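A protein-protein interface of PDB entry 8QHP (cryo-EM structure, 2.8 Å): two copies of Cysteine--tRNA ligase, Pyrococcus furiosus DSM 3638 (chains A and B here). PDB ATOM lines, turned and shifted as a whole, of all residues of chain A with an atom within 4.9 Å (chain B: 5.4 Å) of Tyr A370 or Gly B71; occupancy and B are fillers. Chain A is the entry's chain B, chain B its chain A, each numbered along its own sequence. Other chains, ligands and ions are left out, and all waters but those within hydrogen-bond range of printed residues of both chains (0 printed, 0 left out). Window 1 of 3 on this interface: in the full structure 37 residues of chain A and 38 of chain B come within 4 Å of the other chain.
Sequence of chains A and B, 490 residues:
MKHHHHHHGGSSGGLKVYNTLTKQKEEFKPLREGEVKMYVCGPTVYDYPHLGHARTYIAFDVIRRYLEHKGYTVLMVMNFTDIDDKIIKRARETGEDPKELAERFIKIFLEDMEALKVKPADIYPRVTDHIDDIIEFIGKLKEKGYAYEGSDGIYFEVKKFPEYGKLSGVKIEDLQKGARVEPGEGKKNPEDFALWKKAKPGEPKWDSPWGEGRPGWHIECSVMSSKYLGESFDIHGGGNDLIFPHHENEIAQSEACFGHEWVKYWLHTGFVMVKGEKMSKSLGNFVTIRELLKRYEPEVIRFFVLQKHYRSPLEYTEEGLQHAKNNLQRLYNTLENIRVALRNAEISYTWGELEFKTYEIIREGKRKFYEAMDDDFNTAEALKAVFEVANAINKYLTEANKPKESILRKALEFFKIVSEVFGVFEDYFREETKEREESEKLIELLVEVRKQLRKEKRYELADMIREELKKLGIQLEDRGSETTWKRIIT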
ATOM      1  N   TYR A  66      -6.094 -10.980  15.283  1.00  0.00           N
ATOM      2  CA  TYR A  66      -7.341 -11.348  15.945  1.00  0.00           C
ATOM      3  C   TYR A  66      -7.086 -11.907  17.339  1.00  0.00           C
ATOM      4  O   TYR A  66      -7.842 -11.620  18.273  1.00  0.00           O
ATOM      5  CB  TYR A  66      -8.121 -12.355  15.105  1.00  0.00           C
ATOM      6  CG  TYR A  66      -9.478 -12.657  15.690  1.00  0.00           C
ATOM      7  CD1 TYR A  66     -10.453 -11.673  15.759  1.00  0.00           C
ATOM      8  CD2 TYR A  66      -9.783 -13.917  16.183  1.00  0.00           C
ATOM      9  CE1 TYR A  66     -11.691 -11.934  16.298  1.00  0.00           C
ATOM     10  CE2 TYR A  66     -11.023 -14.187  16.722  1.00  0.00           C
ATOM     11  CZ  TYR A  66     -11.973 -13.192  16.776  1.00  0.00           C
ATOM     12  OH  TYR A  66     -13.211 -13.454  17.312  1.00  0.00           O
ATOM     13  N   HIS A  69      -6.445  -9.105  19.494  1.00  0.00           N
ATOM     14  CA  HIS A  69      -7.673  -8.339  19.665  1.00  0.00           C
ATOM     15  C   HIS A  69      -8.583  -8.962  20.714  1.00  0.00           C
ATOM     16  O   HIS A  69      -9.382  -8.256  21.337  1.00  0.00           O
ATOM     17  CB  HIS A  69      -8.398  -8.226  18.325  1.00  0.00           C
ATOM     18  CG  HIS A  69      -9.677  -7.452  18.390  1.00  0.00           C
ATOM     19  ND1 HIS A  69      -9.712  -6.076  18.433  1.00  0.00           N
ATOM     20  CD2 HIS A  69     -10.965  -7.863  18.411  1.00  0.00           C
ATOM     21  CE1 HIS A  69     -10.969  -5.672  18.481  1.00  0.00           C
ATOM     22  NE2 HIS A  69     -11.749  -6.737  18.468  1.00  0.00           N
ATOM     23  N   LYS A 366     -21.383  -6.332  13.591  1.00  0.00           N
ATOM     24  CA  LYS A 366     -20.275  -6.597  14.506  1.00  0.00           C
ATOM     25  C   LYS A 366     -20.387  -7.990  15.111  1.00  0.00           C
ATOM     26  O   LYS A 366     -19.386  -8.712  15.229  1.00  0.00           O
ATOM     27  CB  LYS A 366     -20.220  -5.542  15.610  1.00  0.00           C
ATOM     28  CG  LYS A 366     -19.226  -5.892  16.708  1.00  0.00           C
ATOM     29  CD  LYS A 366     -19.259  -4.911  17.864  1.00  0.00           C
ATOM     30  CE  LYS A 366     -18.470  -3.655  17.559  1.00  0.00           C
ATOM     31  NZ  LYS A 366     -18.384  -2.765  18.744  1.00  0.00           N
ATOM     32  N   ARG A 367     -21.602  -8.387  15.497  1.00  0.00           N
ATOM     33  CA  ARG A 367     -21.794  -9.712  16.074  1.00  0.00           C
ATOM     34  C   ARG A 367     -21.427 -10.800  15.074  1.00  0.00           C
ATOM     35  O   ARG A 367     -20.754 -11.777  15.420  1.00  0.00           O
ATOM     36  CB  ARG A 367     -23.238  -9.876  16.543  1.00  0.00           C
ATOM     37  CG  ARG A 367     -23.447 -11.059  17.467  1.00  0.00           C
ATOM     38  CD  ARG A 367     -24.915 -11.411  17.577  1.00  0.00           C
ATOM     39  NE  ARG A 367     -25.449 -11.856  16.297  1.00  0.00           N
ATOM     40  CZ  ARG A 367     -25.365 -13.098  15.843  1.00  0.00           C
ATOM     41  NH1 ARG A 367     -24.776 -14.051  16.546  1.00  0.00           N
ATOM     42  NH2 ARG A 367     -25.884 -13.390  14.655  1.00  0.00           N
ATOM     43  N   LYS A 368     -21.855 -10.645  13.818  1.00  0.00           N
ATOM     44  CA  LYS A 368     -21.538 -11.640  12.800  1.00  0.00           C
ATOM     45  C   LYS A 368     -20.061 -11.619  12.435  1.00  0.00           C
ATOM     46  O   LYS A 368     -19.499 -12.663  12.096  1.00  0.00           O
ATOM     47  CB  LYS A 368     -22.392 -11.416  11.554  1.00  0.00           C
ATOM     48  CG  LYS A 368     -23.862 -11.720  11.751  1.00  0.00           C
ATOM     49  CD  LYS A 368     -24.457 -12.345  10.503  1.00  0.00           C
ATOM     50  CE  LYS A 368     -24.204 -11.489   9.274  1.00  0.00           C
ATOM     51  NZ  LYS A 368     -24.884 -10.169   9.362  1.00  0.00           N
ATOM     52  N   PHE A 369     -19.415 -10.455  12.511  1.00  0.00           N
ATOM     53  CA  PHE A 369     -17.974 -10.390  12.299  1.00  0.00           C
ATOM     54  C   PHE A 369     -17.238 -11.196  13.358  1.00  0.00           C
ATOM     55  O   PHE A 369     -16.343 -11.991  13.044  1.00  0.00           O
ATOM     56  CB  PHE A 369     -17.521  -8.929  12.309  1.00  0.00           C
ATOM     57  CG  PHE A 369     -16.034  -8.745  12.196  1.00  0.00           C
ATOM     58  CD1 PHE A 369     -15.428  -8.635  10.959  1.00  0.00           C
ATOM     59  CD2 PHE A 369     -15.243  -8.657  13.330  1.00  0.00           C
ATOM     60  CE1 PHE A 369     -14.062  -8.458  10.852  1.00  0.00           C
ATOM     61  CE2 PHE A 369     -13.878  -8.481  13.229  1.00  0.00           C
ATOM     62  CZ  PHE A 369     -13.288  -8.381  11.989  1.00  0.00           C
ATOM     63  N   TYR A 370     -17.611 -11.011  14.627  1.00  0.00           N
ATOM     64  CA  TYR A 370     -16.961 -11.770  15.690  1.00  0.00           C
ATOM     65  C   TYR A 370     -17.286 -13.254  15.588  1.00  0.00           C
ATOM     66  O   TYR A 370     -16.423 -14.100  15.842  1.00  0.00           O
ATOM     67  CB  TYR A 370     -17.360 -11.222  17.058  1.00  0.00           C
ATOM     68  CG  TYR A 370     -16.561 -10.011  17.469  1.00  0.00           C
ATOM     69  CD1 TYR A 370     -15.179 -10.067  17.561  1.00  0.00           C
ATOM     70  CD2 TYR A 370     -17.188  -8.813  17.774  1.00  0.00           C
ATOM     71  CE1 TYR A 370     -14.443  -8.965  17.936  1.00  0.00           C
ATOM     72  CE2 TYR A 370     -16.461  -7.706  18.151  1.00  0.00           C
ATOM     73  CZ  TYR A 370     -15.090  -7.787  18.230  1.00  0.00           C
ATOM     74  OH  TYR A 370     -14.362  -6.684  18.607  1.00  0.00           O
ATOM     75  N   GLU A 371     -18.518 -13.591  15.205  1.00  0.00           N
ATOM     76  CA  GLU A 371     -18.889 -14.993  15.053  1.00  0.00           C
ATOM     77  C   GLU A 371     -18.117 -15.652  13.916  1.00  0.00           C
ATOM     78  O   GLU A 371     -17.718 -16.817  14.024  1.00  0.00           O
ATOM     79  CB  GLU A 371     -20.395 -15.111  14.823  1.00  0.00           C
ATOM     80  CG  GLU A 371     -20.893 -16.536  14.660  1.00  0.00           C
ATOM     81  CD  GLU A 371     -22.397 -16.611  14.491  1.00  0.00           C
ATOM     82  OE1 GLU A 371     -23.045 -15.543  14.454  1.00  0.00           O
ATOM     83  OE2 GLU A 371     -22.932 -17.734  14.396  1.00  0.00           O
ATOM     84  N   ALA A 372     -17.905 -14.926  12.816  1.00  0.00           N
ATOM     85  CA  ALA A 372     -17.154 -15.476  11.695  1.00  0.00           C
ATOM     86  C   ALA A 372     -15.680 -15.626  12.035  1.00  0.00           C
ATOM     87  O   ALA A 372     -15.065 -16.649  11.716  1.00  0.00           O
ATOM     88  CB  ALA A 372     -17.330 -14.589  10.466  1.00  0.00           C
ATOM     89  N   MET A 373     -15.091 -14.617  12.681  1.00  0.00           N
ATOM     90  CA  MET A 373     -13.687 -14.715  13.053  1.00  0.00           C
ATOM     91  C   MET A 373     -13.452 -15.744  14.148  1.00  0.00           C
ATOM     92  O   MET A 373     -12.338 -16.264  14.264  1.00  0.00           O
ATOM     93  CB  MET A 373     -13.160 -13.350  13.486  1.00  0.00           C
ATOM     94  CG  MET A 373     -13.087 -12.336  12.361  1.00  0.00           C
ATOM     95  SD  MET A 373     -12.047 -12.898  11.003  1.00  0.00           S
ATOM     96  CE  MET A 373     -10.472 -13.077  11.833  1.00  0.00           C
ATOM     97  N   ASP A 374     -14.472 -16.053  14.953  1.00  0.00           N
ATOM     98  CA  ASP A 374     -14.358 -17.129  15.927  1.00  0.00           C
ATOM     99  C   ASP A 374     -14.506 -18.505  15.298  1.00  0.00           C
ATOM    100  O   ASP A 374     -14.172 -19.505  15.942  1.00  0.00           O
ATOM    101  CB  ASP A 374     -15.403 -16.964  17.032  1.00  0.00           C
ATOM    102  CG  ASP A 374     -15.069 -15.841  17.988  1.00  0.00           C
ATOM    103  OD1 ASP A 374     -13.880 -15.474  18.083  1.00  0.00           O
ATOM    104  OD2 ASP A 374     -15.994 -15.328  18.649  1.00  0.00           O
ATOM    105  N   ILE A 417     -12.454  -1.621  14.302  1.00  0.00           N
ATOM    106  CA  ILE A 417     -12.204  -3.006  14.693  1.00  0.00           C
ATOM    107  C   ILE A 417     -11.793  -3.830  13.478  1.00  0.00           C
ATOM    108  O   ILE A 417     -10.852  -4.634  13.539  1.00  0.00           O
ATOM    109  CB  ILE A 417     -13.443  -3.600  15.388  1.00  0.00           C
ATOM    110  CG1 ILE A 417     -13.628  -2.970  16.768  1.00  0.00           C
ATOM    111  CG2 ILE A 417     -13.324  -5.110  15.497  1.00  0.00           C
ATOM    112  CD1 ILE A 417     -14.786  -3.542  17.548  1.00  0.00           C
ATOM    113  N   GLY B  34     -24.086  -9.793  22.689  1.00  0.00           N
ATOM    114  CA  GLY B  34     -23.317  -8.809  21.963  1.00  0.00           C
ATOM    115  C   GLY B  34     -23.790  -7.381  22.106  1.00  0.00           C
ATOM    116  O   GLY B  34     -23.178  -6.485  21.512  1.00  0.00           O
ATOM    117  N   LEU B  67     -16.632  -2.082  28.127  1.00  0.00           N
ATOM    118  CA  LEU B  67     -17.621  -2.980  27.544  1.00  0.00           C
ATOM    119  C   LEU B  67     -17.476  -3.048  26.029  1.00  0.00           C
ATOM    120  O   LEU B  67     -17.622  -4.123  25.436  1.00  0.00           O
ATOM    121  CB  LEU B  67     -19.030  -2.539  27.930  1.00  0.00           C
ATOM    122  CG  LEU B  67     -19.438  -2.798  29.378  1.00  0.00           C
ATOM    123  CD1 LEU B  67     -20.829  -2.255  29.633  1.00  0.00           C
ATOM    124  CD2 LEU B  67     -19.373  -4.279  29.695  1.00  0.00           C
ATOM    125  N   GLU B  68     -17.197  -1.913  25.385  1.00  0.00           N
ATOM    126  CA  GLU B  68     -16.953  -1.931  23.947  1.00  0.00           C
ATOM    127  C   GLU B  68     -15.639  -2.624  23.612  1.00  0.00           C
ATOM    128  O   GLU B  68     -15.512  -3.227  22.542  1.00  0.00           O
ATOM    129  CB  GLU B  68     -16.955  -0.511  23.390  1.00  0.00           C
ATOM    130  CG  GLU B  68     -18.294   0.188  23.484  1.00  0.00           C
ATOM    131  CD  GLU B  68     -18.218   1.633  23.052  1.00  0.00           C
ATOM    132  OE1 GLU B  68     -17.093   2.172  22.988  1.00  0.00           O
ATOM    133  OE2 GLU B  68     -19.279   2.228  22.774  1.00  0.00           O
ATOM    134  N   HIS B  69     -14.656  -2.544  24.510  1.00  0.00           N
ATOM    135  CA  HIS B  69     -13.375  -3.192  24.269  1.00  0.00           C
ATOM    136  C   HIS B  69     -13.499  -4.708  24.296  1.00  0.00           C
ATOM    137  O   HIS B  69     -12.721  -5.403  23.637  1.00  0.00           O
ATOM    138  CB  HIS B  69     -12.350  -2.724  25.301  1.00  0.00           C
ATOM    139  CG  HIS B  69     -10.994  -3.332  25.127  1.00  0.00           C
ATOM    140  ND1 HIS B  69     -10.099  -2.897  24.174  1.00  0.00           N
ATOM    141  CD2 HIS B  69     -10.378  -4.339  25.789  1.00  0.00           C
ATOM    142  CE1 HIS B  69      -8.992  -3.612  24.255  1.00  0.00           C
ATOM    143  NE2 HIS B  69      -9.135  -4.493  25.228  1.00  0.00           N
ATOM    144  N   LYS B  70     -14.467  -5.237  25.040  1.00  0.00           N
ATOM    145  CA  LYS B  70     -14.661  -6.677  25.124  1.00  0.00           C
ATOM    146  C   LYS B  70     -15.523  -7.227  23.995  1.00  0.00           C
ATOM    147  O   LYS B  70     -15.799  -8.431  23.984  1.00  0.00           O
ATOM    148  CB  LYS B  70     -15.280  -7.054  26.471  1.00  0.00           C
ATOM    149  CG  LYS B  70     -14.388  -6.776  27.661  1.00  0.00           C
ATOM    150  CD  LYS B  70     -14.889  -7.499  28.898  1.00  0.00           C
ATOM    151  CE  LYS B  70     -14.835  -9.009  28.722  1.00  0.00           C
ATOM    152  NZ  LYS B  70     -15.311  -9.718  29.940  1.00  0.00           N
ATOM    153  N   GLY B  71     -15.957  -6.386  23.060  1.00  0.00           N
ATOM    154  CA  GLY B  71     -16.728  -6.832  21.921  1.00  0.00           C
ATOM    155  C   GLY B  71     -18.207  -6.522  21.972  1.00  0.00           C
ATOM    156  O   GLY B  71     -18.918  -6.837  21.011  1.00  0.00           O
ATOM    157  N   TYR B  72     -18.692  -5.916  23.050  1.00  0.00           N
ATOM    158  CA  TYR B  72     -20.099  -5.555  23.134  1.00  0.00           C
ATOM    159  C   TYR B  72     -20.380  -4.291  22.333  1.00  0.00           C
ATOM    160  O   TYR B  72     -19.532  -3.405  22.207  1.00  0.00           O
ATOM    161  CB  TYR B  72     -20.519  -5.335  24.587  1.00  0.00           C
ATOM    162  CG  TYR B  72     -20.444  -6.563  25.461  1.00  0.00           C
ATOM    163  CD1 TYR B  72     -21.459  -7.506  25.449  1.00  0.00           C
ATOM    164  CD2 TYR B  72     -19.369  -6.768  26.310  1.00  0.00           C
ATOM    165  CE1 TYR B  72     -21.400  -8.626  26.251  1.00  0.00           C
ATOM    166  CE2 TYR B  72     -19.301  -7.885  27.116  1.00  0.00           C
ATOM    167  CZ  TYR B  72     -20.320  -8.811  27.082  1.00  0.00           C
ATOM    168  OH  TYR B  72     -20.257  -9.927  27.882  1.00  0.00           O
ATOM    169  N   THR B  73     -21.590  -4.217  21.789  1.00  0.00           N
ATOM    170  CA  THR B  73     -22.116  -2.991  21.205  1.00  0.00           C
ATOM    171  C   THR B  73     -22.948  -2.297  22.273  1.00  0.00           C
ATOM    172  O   THR B  73     -23.963  -2.839  22.720  1.00  0.00           O
ATOM    173  CB  THR B  73     -22.962  -3.281  19.966  1.00  0.00           C
ATOM    174  OG1 THR B  73     -22.164  -3.960  18.990  1.00  0.00           O
ATOM    175  CG2 THR B  73     -23.485  -1.987  19.371  1.00  0.00           C
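Among the printed residues, 4 pairs touch across the chains.
Among the printed residues, merely in contact across the chains: Lys A366 with Thr B73 (3.3 Å), Lys A366 with Tyr B72 (3.7 Å), Lys A366 with Gly B71 (3.7 Å) and Tyr A370 with Gly B71 (3.9 Å).
The backbone carbonyl oxygen of Gly B34 lies within hydrogen-bond range of the backbone NH of Thr B73 (2.8 Å). The backbone NH of Tyr B72 is in hydrogen-bond range of the backbone carbonyl oxygen of Leu B67 (3.2 Å). OH of Tyr A370 sits at hydrogen-bond distance from NE2 of His A69 (2.6 Å).
1 position is printed for both chains. Of the 4 pairs that touch across the chains among the printed residues, none has its exchanged pair printed and touching as well.
Gly B71 touches just these residues of chain A: Lys A366 (3.7 Å) and Tyr A370 (3.9 Å). Printed residues of chain A within 4 Å of Tyr B72: Lys A366 (3.7 Å). Printed residues of chain A within 4 Å of Thr B73: Lys A366.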
